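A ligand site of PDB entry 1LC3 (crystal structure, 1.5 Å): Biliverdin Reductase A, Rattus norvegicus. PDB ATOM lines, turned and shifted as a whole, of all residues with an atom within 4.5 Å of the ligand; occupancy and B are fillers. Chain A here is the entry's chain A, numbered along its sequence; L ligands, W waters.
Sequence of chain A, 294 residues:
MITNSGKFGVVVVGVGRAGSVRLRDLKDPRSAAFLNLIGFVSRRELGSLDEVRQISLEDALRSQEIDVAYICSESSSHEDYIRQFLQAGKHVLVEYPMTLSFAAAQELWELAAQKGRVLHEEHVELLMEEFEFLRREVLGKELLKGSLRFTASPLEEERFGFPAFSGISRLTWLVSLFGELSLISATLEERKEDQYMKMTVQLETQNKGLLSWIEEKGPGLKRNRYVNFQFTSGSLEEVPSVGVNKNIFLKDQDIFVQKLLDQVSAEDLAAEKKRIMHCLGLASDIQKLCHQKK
An oxygen (O1) of the ligand is in hydrogen-bond range of the backbone NH (N) of Arg 17, 3.1 Å away. O12 of the ligand is in hydrogen-bond range of N of Ser 75. O13 of the ligand sits at hydrogen-bond distance from O of Tyr 96, 2.7 Å away. OG of Ser 75 lies within hydrogen-bond range of O12 of the ligand (3.0 Å). N3 of the ligand sits at hydrogen-bond distance from O of Ser 166, 2.9 Å away. An oxygen (O12) of the ligand sits close to a ring nitrogen (NE2) of His 78. The backbone NH (N) of Ala 18 is in hydrogen-bond range of an oxygen (O9) of the ligand (2.7 Å).
N of Ser 75 lies within hydrogen-bond range of O of Arg 159. The backbone carbonyl oxygen (O) of Phe 160 is in hydrogen-bond range of the side-chain hydroxyl (OG) of Ser 75 (3.2 Å). A ring nitrogen (NE2) of His 78 lies within hydrogen-bond range of the backbone carbonyl oxygen of Ser 73 (2.7 Å). ND1 of His 78 lies close to O of Glu 95 (3.3 Å). The side-chain carboxylate of Glu 122 lies close to the side-chain carboxylate of Glu 95 (2.5 Å). The side-chain carboxylate of Glu 95 lies within hydrogen-bond range of the side-chain sulfur of Cys 72 (3.5 Å). ND1 of His 78 sits at hydrogen-bond distance from O of Pro 97 (2.7 Å).
Residues that only touch the ligand: Ser 73, Glu 122, Phe 160, Glu 95, Leu 155, Pro 97, Phe 249, Gly 16 and Cys 72.
Water W4 lies within hydrogen-bond range of a nitrogen (N4) of the ligand, the side-chain amino group (NZ) of Lys 217 and the side-chain hydroxyl (OG) of Ser 166. Water W3 lies within hydrogen-bond range of an oxygen (O2) of the ligand (3.0 Å) and the guanidinium group of Arg 159 (3.3 Å).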
ATOM      1  N   GLY A  16     -23.452   0.556  12.201  1.00  0.00           N
ATOM      2  CA  GLY A  16     -22.209   0.261  12.878  1.00  0.00           C
ATOM      3  C   GLY A  16     -22.206   1.191  14.083  1.00  0.00           C
ATOM      4  O   GLY A  16     -23.280   1.515  14.605  1.00  0.00           O
ATOM      5  N   ARG A  17     -21.040   1.666  14.490  1.00  0.00           N
ATOM      6  CA  ARG A  17     -20.960   2.558  15.647  1.00  0.00           C
ATOM      7  C   ARG A  17     -21.719   3.851  15.401  1.00  0.00           C
ATOM      8  O   ARG A  17     -22.578   4.245  16.201  1.00  0.00           O
ATOM      9  CB  ARG A  17     -19.489   2.891  15.945  1.00  0.00           C
ATOM     10  CG  ARG A  17     -19.274   3.590  17.284  1.00  0.00           C
ATOM     11  CD  ARG A  17     -19.483   2.625  18.442  1.00  0.00           C
ATOM     12  NE  ARG A  17     -18.482   1.562  18.419  1.00  0.00           N
ATOM     13  CZ  ARG A  17     -17.209   1.729  18.751  1.00  0.00           C
ATOM     14  NH1 ARG A  17     -16.772   2.916  19.147  1.00  0.00           N
ATOM     15  NH2 ARG A  17     -16.357   0.707  18.681  1.00  0.00           N
ATOM     16  N   ALA A  18     -21.410   4.526  14.295  1.00  0.00           N
ATOM     17  CA  ALA A  18     -22.061   5.790  13.969  1.00  0.00           C
ATOM     18  C   ALA A  18     -23.573   5.620  13.802  1.00  0.00           C
ATOM     19  O   ALA A  18     -24.345   6.420  14.325  1.00  0.00           O
ATOM     20  CB  ALA A  18     -21.460   6.379  12.695  1.00  0.00           C
ATOM     21  N   GLY A  19     -23.976   4.584  13.083  1.00  0.00           N
ATOM     22  CA  GLY A  19     -25.396   4.347  12.866  1.00  0.00           C
ATOM     23  C   GLY A  19     -26.147   4.102  14.166  1.00  0.00           C
ATOM     24  O   GLY A  19     -27.264   4.577  14.336  1.00  0.00           O
ATOM     25  N   CYS A  72     -24.360   6.266   7.268  1.00  0.00           N
ATOM     26  CA  CYS A  72     -23.405   5.908   8.316  1.00  0.00           C
ATOM     27  C   CYS A  72     -22.596   4.629   8.047  1.00  0.00           C
ATOM     28  O   CYS A  72     -21.980   4.076   8.957  1.00  0.00           O
ATOM     29  CB  CYS A  72     -24.163   5.732   9.642  1.00  0.00           C
ATOM     30  SG  CYS A  72     -25.212   7.139  10.086  1.00  0.00           S
ATOM     31  N   SER A  73     -22.608   4.186   6.796  1.00  0.00           N
ATOM     32  CA  SER A  73     -21.870   2.978   6.405  1.00  0.00           C
ATOM     33  C   SER A  73     -20.380   3.266   6.305  1.00  0.00           C
ATOM     34  O   SER A  73     -19.942   4.398   6.527  1.00  0.00           O
ATOM     35  CB  SER A  73     -22.391   2.482   5.055  1.00  0.00           C
ATOM     36  OG  SER A  73     -22.306   3.507   4.080  1.00  0.00           O
ATOM     37  N   GLU A  74     -19.574   2.257   5.979  1.00  0.00           N
ATOM     38  CA  GLU A  74     -18.145   2.503   5.867  1.00  0.00           C
ATOM     39  C   GLU A  74     -17.882   3.474   4.716  1.00  0.00           C
ATOM     40  O   GLU A  74     -18.671   3.555   3.765  1.00  0.00           O
ATOM     41  CB  GLU A  74     -17.350   1.203   5.643  1.00  0.00           C
ATOM     42  CG  GLU A  74     -17.582   0.541   4.312  1.00  0.00           C
ATOM     43  CD  GLU A  74     -18.916  -0.152   4.225  1.00  0.00           C
ATOM     44  OE1 GLU A  74     -19.275  -0.610   3.126  1.00  0.00           O
ATOM     45  OE2 GLU A  74     -19.584  -0.257   5.275  1.00  0.00           O
ATOM     46  N   SER A  75     -16.786   4.201   4.828  1.00  0.00           N
ATOM     47  CA  SER A  75     -16.415   5.215   3.844  1.00  0.00           C
ATOM     48  C   SER A  75     -16.529   4.817   2.389  1.00  0.00           C
ATOM     49  O   SER A  75     -17.039   5.580   1.575  1.00  0.00           O
ATOM     50  CB  SER A  75     -14.987   5.690   4.125  1.00  0.00           C
ATOM     51  OG  SER A  75     -14.849   6.044   5.485  1.00  0.00           O
ATOM     52  N   HIS A  78     -20.024   5.292   0.820  1.00  0.00           N
ATOM     53  CA  HIS A  78     -20.719   6.574   0.899  1.00  0.00           C
ATOM     54  C   HIS A  78     -21.168   7.144  -0.431  1.00  0.00           C
ATOM     55  O   HIS A  78     -22.329   7.528  -0.589  1.00  0.00           O
ATOM     56  CB  HIS A  78     -19.846   7.624   1.590  1.00  0.00           C
ATOM     57  CG  HIS A  78     -19.683   7.386   3.058  1.00  0.00           C
ATOM     58  ND1 HIS A  78     -18.946   8.236   3.859  1.00  0.00           N
ATOM     59  CD2 HIS A  78     -20.150   6.414   3.868  1.00  0.00           C
ATOM     60  CE1 HIS A  78     -18.968   7.793   5.108  1.00  0.00           C
ATOM     61  NE2 HIS A  78     -19.695   6.686   5.133  1.00  0.00           N
ATOM     62  N   GLU A  95     -21.616  10.821   7.214  1.00  0.00           N
ATOM     63  CA  GLU A  95     -20.472  10.968   8.098  1.00  0.00           C
ATOM     64  C   GLU A  95     -19.222  11.151   7.236  1.00  0.00           C
ATOM     65  O   GLU A  95     -19.150  10.619   6.126  1.00  0.00           O
ATOM     66  CB  GLU A  95     -20.317   9.727   8.981  1.00  0.00           C
ATOM     67  CG  GLU A  95     -21.590   9.199   9.637  1.00  0.00           C
ATOM     68  CD  GLU A  95     -22.252  10.132  10.648  1.00  0.00           C
ATOM     69  OE1 GLU A  95     -23.201   9.680  11.320  1.00  0.00           O
ATOM     70  OE2 GLU A  95     -21.830  11.316  10.776  1.00  0.00           O
ATOM     71  N   TYR A  96     -18.251  11.916   7.710  1.00  0.00           N
ATOM     72  CA  TYR A  96     -17.040  12.117   6.913  1.00  0.00           C
ATOM     73  C   TYR A  96     -16.285  10.809   6.817  1.00  0.00           C
ATOM     74  O   TYR A  96     -16.364   9.964   7.707  1.00  0.00           O
ATOM     75  CB  TYR A  96     -16.149  13.207   7.533  1.00  0.00           C
ATOM     76  CG  TYR A  96     -15.360  12.789   8.767  1.00  0.00           C
ATOM     77  CD1 TYR A  96     -14.264  11.939   8.665  1.00  0.00           C
ATOM     78  CD2 TYR A  96     -15.705  13.289  10.026  1.00  0.00           C
ATOM     79  CE1 TYR A  96     -13.529  11.578   9.789  1.00  0.00           C
ATOM     80  CE2 TYR A  96     -14.961  12.943  11.154  1.00  0.00           C
ATOM     81  CZ  TYR A  96     -13.879  12.084  11.036  1.00  0.00           C
ATOM     82  OH  TYR A  96     -13.152  11.751  12.151  1.00  0.00           O
ATOM     83  N   PRO A  97     -15.564  10.589   5.704  1.00  0.00           N
ATOM     84  CA  PRO A  97     -15.445  11.478   4.547  1.00  0.00           C
ATOM     85  C   PRO A  97     -16.631  11.197   3.610  1.00  0.00           C
ATOM     86  O   PRO A  97     -16.998  10.031   3.428  1.00  0.00           O
ATOM     87  CB  PRO A  97     -14.097  11.081   3.943  1.00  0.00           C
ATOM     88  CG  PRO A  97     -14.062   9.610   4.207  1.00  0.00           C
ATOM     89  CD  PRO A  97     -14.594   9.489   5.618  1.00  0.00           C
ATOM     90  N   GLU A 122     -20.996  15.490   7.978  1.00  0.00           N
ATOM     91  CA  GLU A 122     -20.762  15.666   9.409  1.00  0.00           C
ATOM     92  C   GLU A 122     -19.285  15.824   9.732  1.00  0.00           C
ATOM     93  O   GLU A 122     -18.443  15.095   9.223  1.00  0.00           O
ATOM     94  CB  GLU A 122     -21.349  14.479  10.183  1.00  0.00           C
ATOM     95  CG  GLU A 122     -20.768  14.252  11.593  1.00  0.00           C
ATOM     96  CD  GLU A 122     -19.485  13.435  11.565  1.00  0.00           C
ATOM     97  OE1 GLU A 122     -19.527  12.287  11.051  1.00  0.00           O
ATOM     98  OE2 GLU A 122     -18.445  13.912  12.046  1.00  0.00           O
ATOM     99  N   LEU A 155      -6.346   0.472  10.629  1.00  0.00           N
ATOM    100  CA  LEU A 155      -7.668   0.685  10.052  1.00  0.00           C
ATOM    101  C   LEU A 155      -7.660   0.178   8.615  1.00  0.00           C
ATOM    102  O   LEU A 155      -6.761   0.510   7.841  1.00  0.00           O
ATOM    103  CB  LEU A 155      -7.997   2.176  10.083  1.00  0.00           C
ATOM    104  CG  LEU A 155      -9.428   2.591   9.730  1.00  0.00           C
ATOM    105  CD1 LEU A 155     -10.390   2.102  10.819  1.00  0.00           C
ATOM    106  CD2 LEU A 155      -9.496   4.107   9.614  1.00  0.00           C
ATOM    107  N   ARG A 159     -11.955  -0.255   3.426  1.00  0.00           N
ATOM    108  CA  ARG A 159     -13.274   0.132   3.923  1.00  0.00           C
ATOM    109  C   ARG A 159     -13.371   1.587   4.351  1.00  0.00           C
ATOM    110  O   ARG A 159     -14.350   2.267   4.018  1.00  0.00           O
ATOM    111  CB  ARG A 159     -13.666  -0.765   5.109  1.00  0.00           C
ATOM    112  CG  ARG A 159     -13.930  -2.220   4.738  1.00  0.00           C
ATOM    113  CD  ARG A 159     -14.167  -3.055   5.991  1.00  0.00           C
ATOM    114  NE  ARG A 159     -15.256  -2.549   6.815  1.00  0.00           N
ATOM    115  CZ  ARG A 159     -16.543  -2.527   6.451  1.00  0.00           C
ATOM    116  NH1 ARG A 159     -16.900  -2.985   5.252  1.00  0.00           N
ATOM    117  NH2 ARG A 159     -17.462  -2.043   7.265  1.00  0.00           N
ATOM    118  N   PHE A 160     -12.370   2.072   5.074  1.00  0.00           N
ATOM    119  CA  PHE A 160     -12.415   3.440   5.557  1.00  0.00           C
ATOM    120  C   PHE A 160     -11.633   4.457   4.745  1.00  0.00           C
ATOM    121  O   PHE A 160     -11.722   5.657   5.004  1.00  0.00           O
ATOM    122  CB  PHE A 160     -11.976   3.478   7.027  1.00  0.00           C
ATOM    123  CG  PHE A 160     -12.837   2.641   7.918  1.00  0.00           C
ATOM    124  CD1 PHE A 160     -12.536   1.298   8.155  1.00  0.00           C
ATOM    125  CD2 PHE A 160     -13.998   3.173   8.470  1.00  0.00           C
ATOM    126  CE1 PHE A 160     -13.383   0.506   8.921  1.00  0.00           C
ATOM    127  CE2 PHE A 160     -14.854   2.381   9.232  1.00  0.00           C
ATOM    128  CZ  PHE A 160     -14.540   1.045   9.466  1.00  0.00           C
ATOM    129  N   SER A 166      -9.500   8.982   5.738  1.00  0.00           N
ATOM    130  CA  SER A 166     -10.028   8.467   7.002  1.00  0.00           C
ATOM    131  C   SER A 166      -9.725   9.421   8.150  1.00  0.00           C
ATOM    132  O   SER A 166     -10.493   9.511   9.098  1.00  0.00           O
ATOM    133  CB  SER A 166      -9.446   7.080   7.299  1.00  0.00           C
ATOM    134  OG  SER A 166      -8.067   7.163   7.618  1.00  0.00           O
ATOM    135  N   LYS A 217      -0.517   4.717  12.386  1.00  0.00           N
ATOM    136  CA  LYS A 217      -1.382   3.626  12.818  1.00  0.00           C
ATOM    137  C   LYS A 217      -0.552   2.364  13.001  1.00  0.00           C
ATOM    138  O   LYS A 217       0.300   2.051  12.167  1.00  0.00           O
ATOM    139  CB  LYS A 217      -2.506   3.375  11.813  1.00  0.00           C
ATOM    140  CG  LYS A 217      -3.456   4.541  11.624  1.00  0.00           C
ATOM    141  CD  LYS A 217      -4.593   4.165  10.691  1.00  0.00           C
ATOM    142  CE  LYS A 217      -5.447   5.386  10.317  1.00  0.00           C
ATOM    143  NZ  LYS A 217      -6.086   6.016  11.509  1.00  0.00           N
ATOM    144  N   ARG A 223      -4.627   5.733  21.186  1.00  0.00           N
ATOM    145  CA  ARG A 223      -5.152   6.882  20.463  1.00  0.00           C
ATOM    146  C   ARG A 223      -4.635   8.149  21.127  1.00  0.00           C
ATOM    147  O   ARG A 223      -5.106   8.540  22.195  1.00  0.00           O
ATOM    148  CB  ARG A 223      -6.686   6.841  20.477  1.00  0.00           C
ATOM    149  CG  ARG A 223      -7.348   7.958  19.694  1.00  0.00           C
ATOM    150  CD  ARG A 223      -8.850   7.726  19.593  1.00  0.00           C
ATOM    151  NE  ARG A 223      -9.168   6.495  18.884  1.00  0.00           N
ATOM    152  CZ  ARG A 223     -10.391   6.039  18.690  1.00  0.00           C
ATOM    153  NH1 ARG A 223     -11.437   6.712  19.153  1.00  0.00           N
ATOM    154  NH2 ARG A 223     -10.579   4.897  18.028  1.00  0.00           N
ATOM    155  N   PHE A 249     -22.766  14.455  18.719  1.00  0.00           N
ATOM    156  CA  PHE A 249     -23.459  14.125  17.487  1.00  0.00           C
ATOM    157  C   PHE A 249     -24.816  14.823  17.415  1.00  0.00           C
ATOM    158  O   PHE A 249     -25.285  15.142  16.317  1.00  0.00           O
ATOM    159  CB  PHE A 249     -23.582  12.607  17.296  1.00  0.00           C
ATOM    160  CG  PHE A 249     -22.293  11.961  16.833  1.00  0.00           C
ATOM    161  CD1 PHE A 249     -21.342  11.541  17.756  1.00  0.00           C
ATOM    162  CD2 PHE A 249     -22.006  11.856  15.480  1.00  0.00           C
ATOM    163  CE1 PHE A 249     -20.128  11.003  17.330  1.00  0.00           C
ATOM    164  CE2 PHE A 249     -20.787  11.325  15.046  1.00  0.00           C
ATOM    165  CZ  PHE A 249     -19.848  10.899  15.971  1.00  0.00           C
HETATM  166  P1  LIG L   1     -17.497   0.827  12.275  1.00  0.00           P
HETATM  167  O1  LIG L   1     -18.444   0.452  13.369  1.00  0.00           O
HETATM  168  O2  LIG L   1     -17.400  -0.246  11.189  1.00  0.00           O
HETATM  169  O3  LIG L   1     -16.108   1.155  12.850  1.00  0.00           O
HETATM  170  C1  LIG L   1     -15.215   0.161  13.510  1.00  0.00           C
HETATM  171  C2  LIG L   1     -14.041   0.813  14.142  1.00  0.00           C
HETATM  172  O4  LIG L   1     -13.405   1.783  13.226  1.00  0.00           O
HETATM  173  C3  LIG L   1     -14.267   1.647  15.466  1.00  0.00           C
HETATM  174  O5  LIG L   1     -13.193   1.343  16.427  1.00  0.00           O
HETATM  175  C4  LIG L   1     -14.282   3.082  15.054  1.00  0.00           C
HETATM  176  O6  LIG L   1     -14.070   4.033  16.022  1.00  0.00           O
HETATM  177  C5  LIG L   1     -13.252   2.977  13.882  1.00  0.00           C
HETATM  178  N1  LIG L   1     -13.394   3.985  12.881  1.00  0.00           N
HETATM  179  C6  LIG L   1     -14.450   4.310  12.061  1.00  0.00           C
HETATM  180  N2  LIG L   1     -14.240   5.309  11.232  1.00  0.00           N
HETATM  181  C7  LIG L   1     -12.956   5.729  11.486  1.00  0.00           C
HETATM  182  C8  LIG L   1     -12.120   6.837  10.867  1.00  0.00           C
HETATM  183  N3  LIG L   1     -12.505   7.661   9.917  1.00  0.00           N
HETATM  184  N4  LIG L   1     -10.809   6.937  11.435  1.00  0.00           N
HETATM  185  C9  LIG L   1     -10.309   6.161  12.404  1.00  0.00           C
HETATM  186  N5  LIG L   1     -11.075   5.112  12.997  1.00  0.00           N
HETATM  187  C10 LIG L   1     -12.414   4.930  12.502  1.00  0.00           C
HETATM  188  O7  LIG L   1     -18.155   2.113  11.665  1.00  0.00           O
HETATM  189  P2  LIG L   1     -18.300   3.652  12.166  1.00  0.00           P
HETATM  190  O8  LIG L   1     -17.526   3.963  13.342  1.00  0.00           O
HETATM  191  O9  LIG L   1     -19.765   3.682  12.294  1.00  0.00           O
HETATM  192  O10 LIG L   1     -18.108   4.696  11.010  1.00  0.00           O
HETATM  193  C11 LIG L   1     -18.227   4.438   9.629  1.00  0.00           C
HETATM  194  C12 LIG L   1     -18.311   5.703   8.878  1.00  0.00           C
HETATM  195  O11 LIG L   1     -18.515   6.869   9.883  1.00  0.00           O
HETATM  196  C13 LIG L   1     -16.944   6.129   8.229  1.00  0.00           C
HETATM  197  O12 LIG L   1     -17.269   6.766   7.096  1.00  0.00           O
HETATM  198  C14 LIG L   1     -16.260   6.994   9.313  1.00  0.00           C
HETATM  199  O13 LIG L   1     -15.226   7.756   8.823  1.00  0.00           O
HETATM  200  C15 LIG L   1     -17.450   7.782   9.795  1.00  0.00           C
HETATM  201  N6  LIG L   1     -17.329   8.478  11.135  1.00  0.00           N
HETATM  202  C16 LIG L   1     -17.350   7.746  12.367  1.00  0.00           C
HETATM  203  C17 LIG L   1     -17.241   8.551  13.482  1.00  0.00           C
HETATM  204  C18 LIG L   1     -17.271   7.674  14.841  1.00  0.00           C
HETATM  205  O14 LIG L   1     -17.169   8.296  15.924  1.00  0.00           O
HETATM  206  N7  LIG L   1     -17.399   6.281  14.726  1.00  0.00           N
HETATM  207  C19 LIG L   1     -17.102   9.972  13.498  1.00  0.00           C
HETATM  208  C20 LIG L   1     -17.094  10.577  12.180  1.00  0.00           C
HETATM  209  C21 LIG L   1     -17.205   9.834  11.004  1.00  0.00           C
HETATM  210  O   HOH W   1     -22.295   2.946  11.382  1.00  0.00           O
HETATM  211  O   HOH W   2     -18.311  -1.575  14.924  1.00  0.00           O
HETATM  212  O   HOH W   3     -19.347   0.080   8.953  1.00  0.00           O
HETATM  213  O   HOH W   4      -8.176   7.810  10.598  1.00  0.00           O
HETATM  214  O   HOH W   5      -9.452   3.882  14.799  1.00  0.00           O
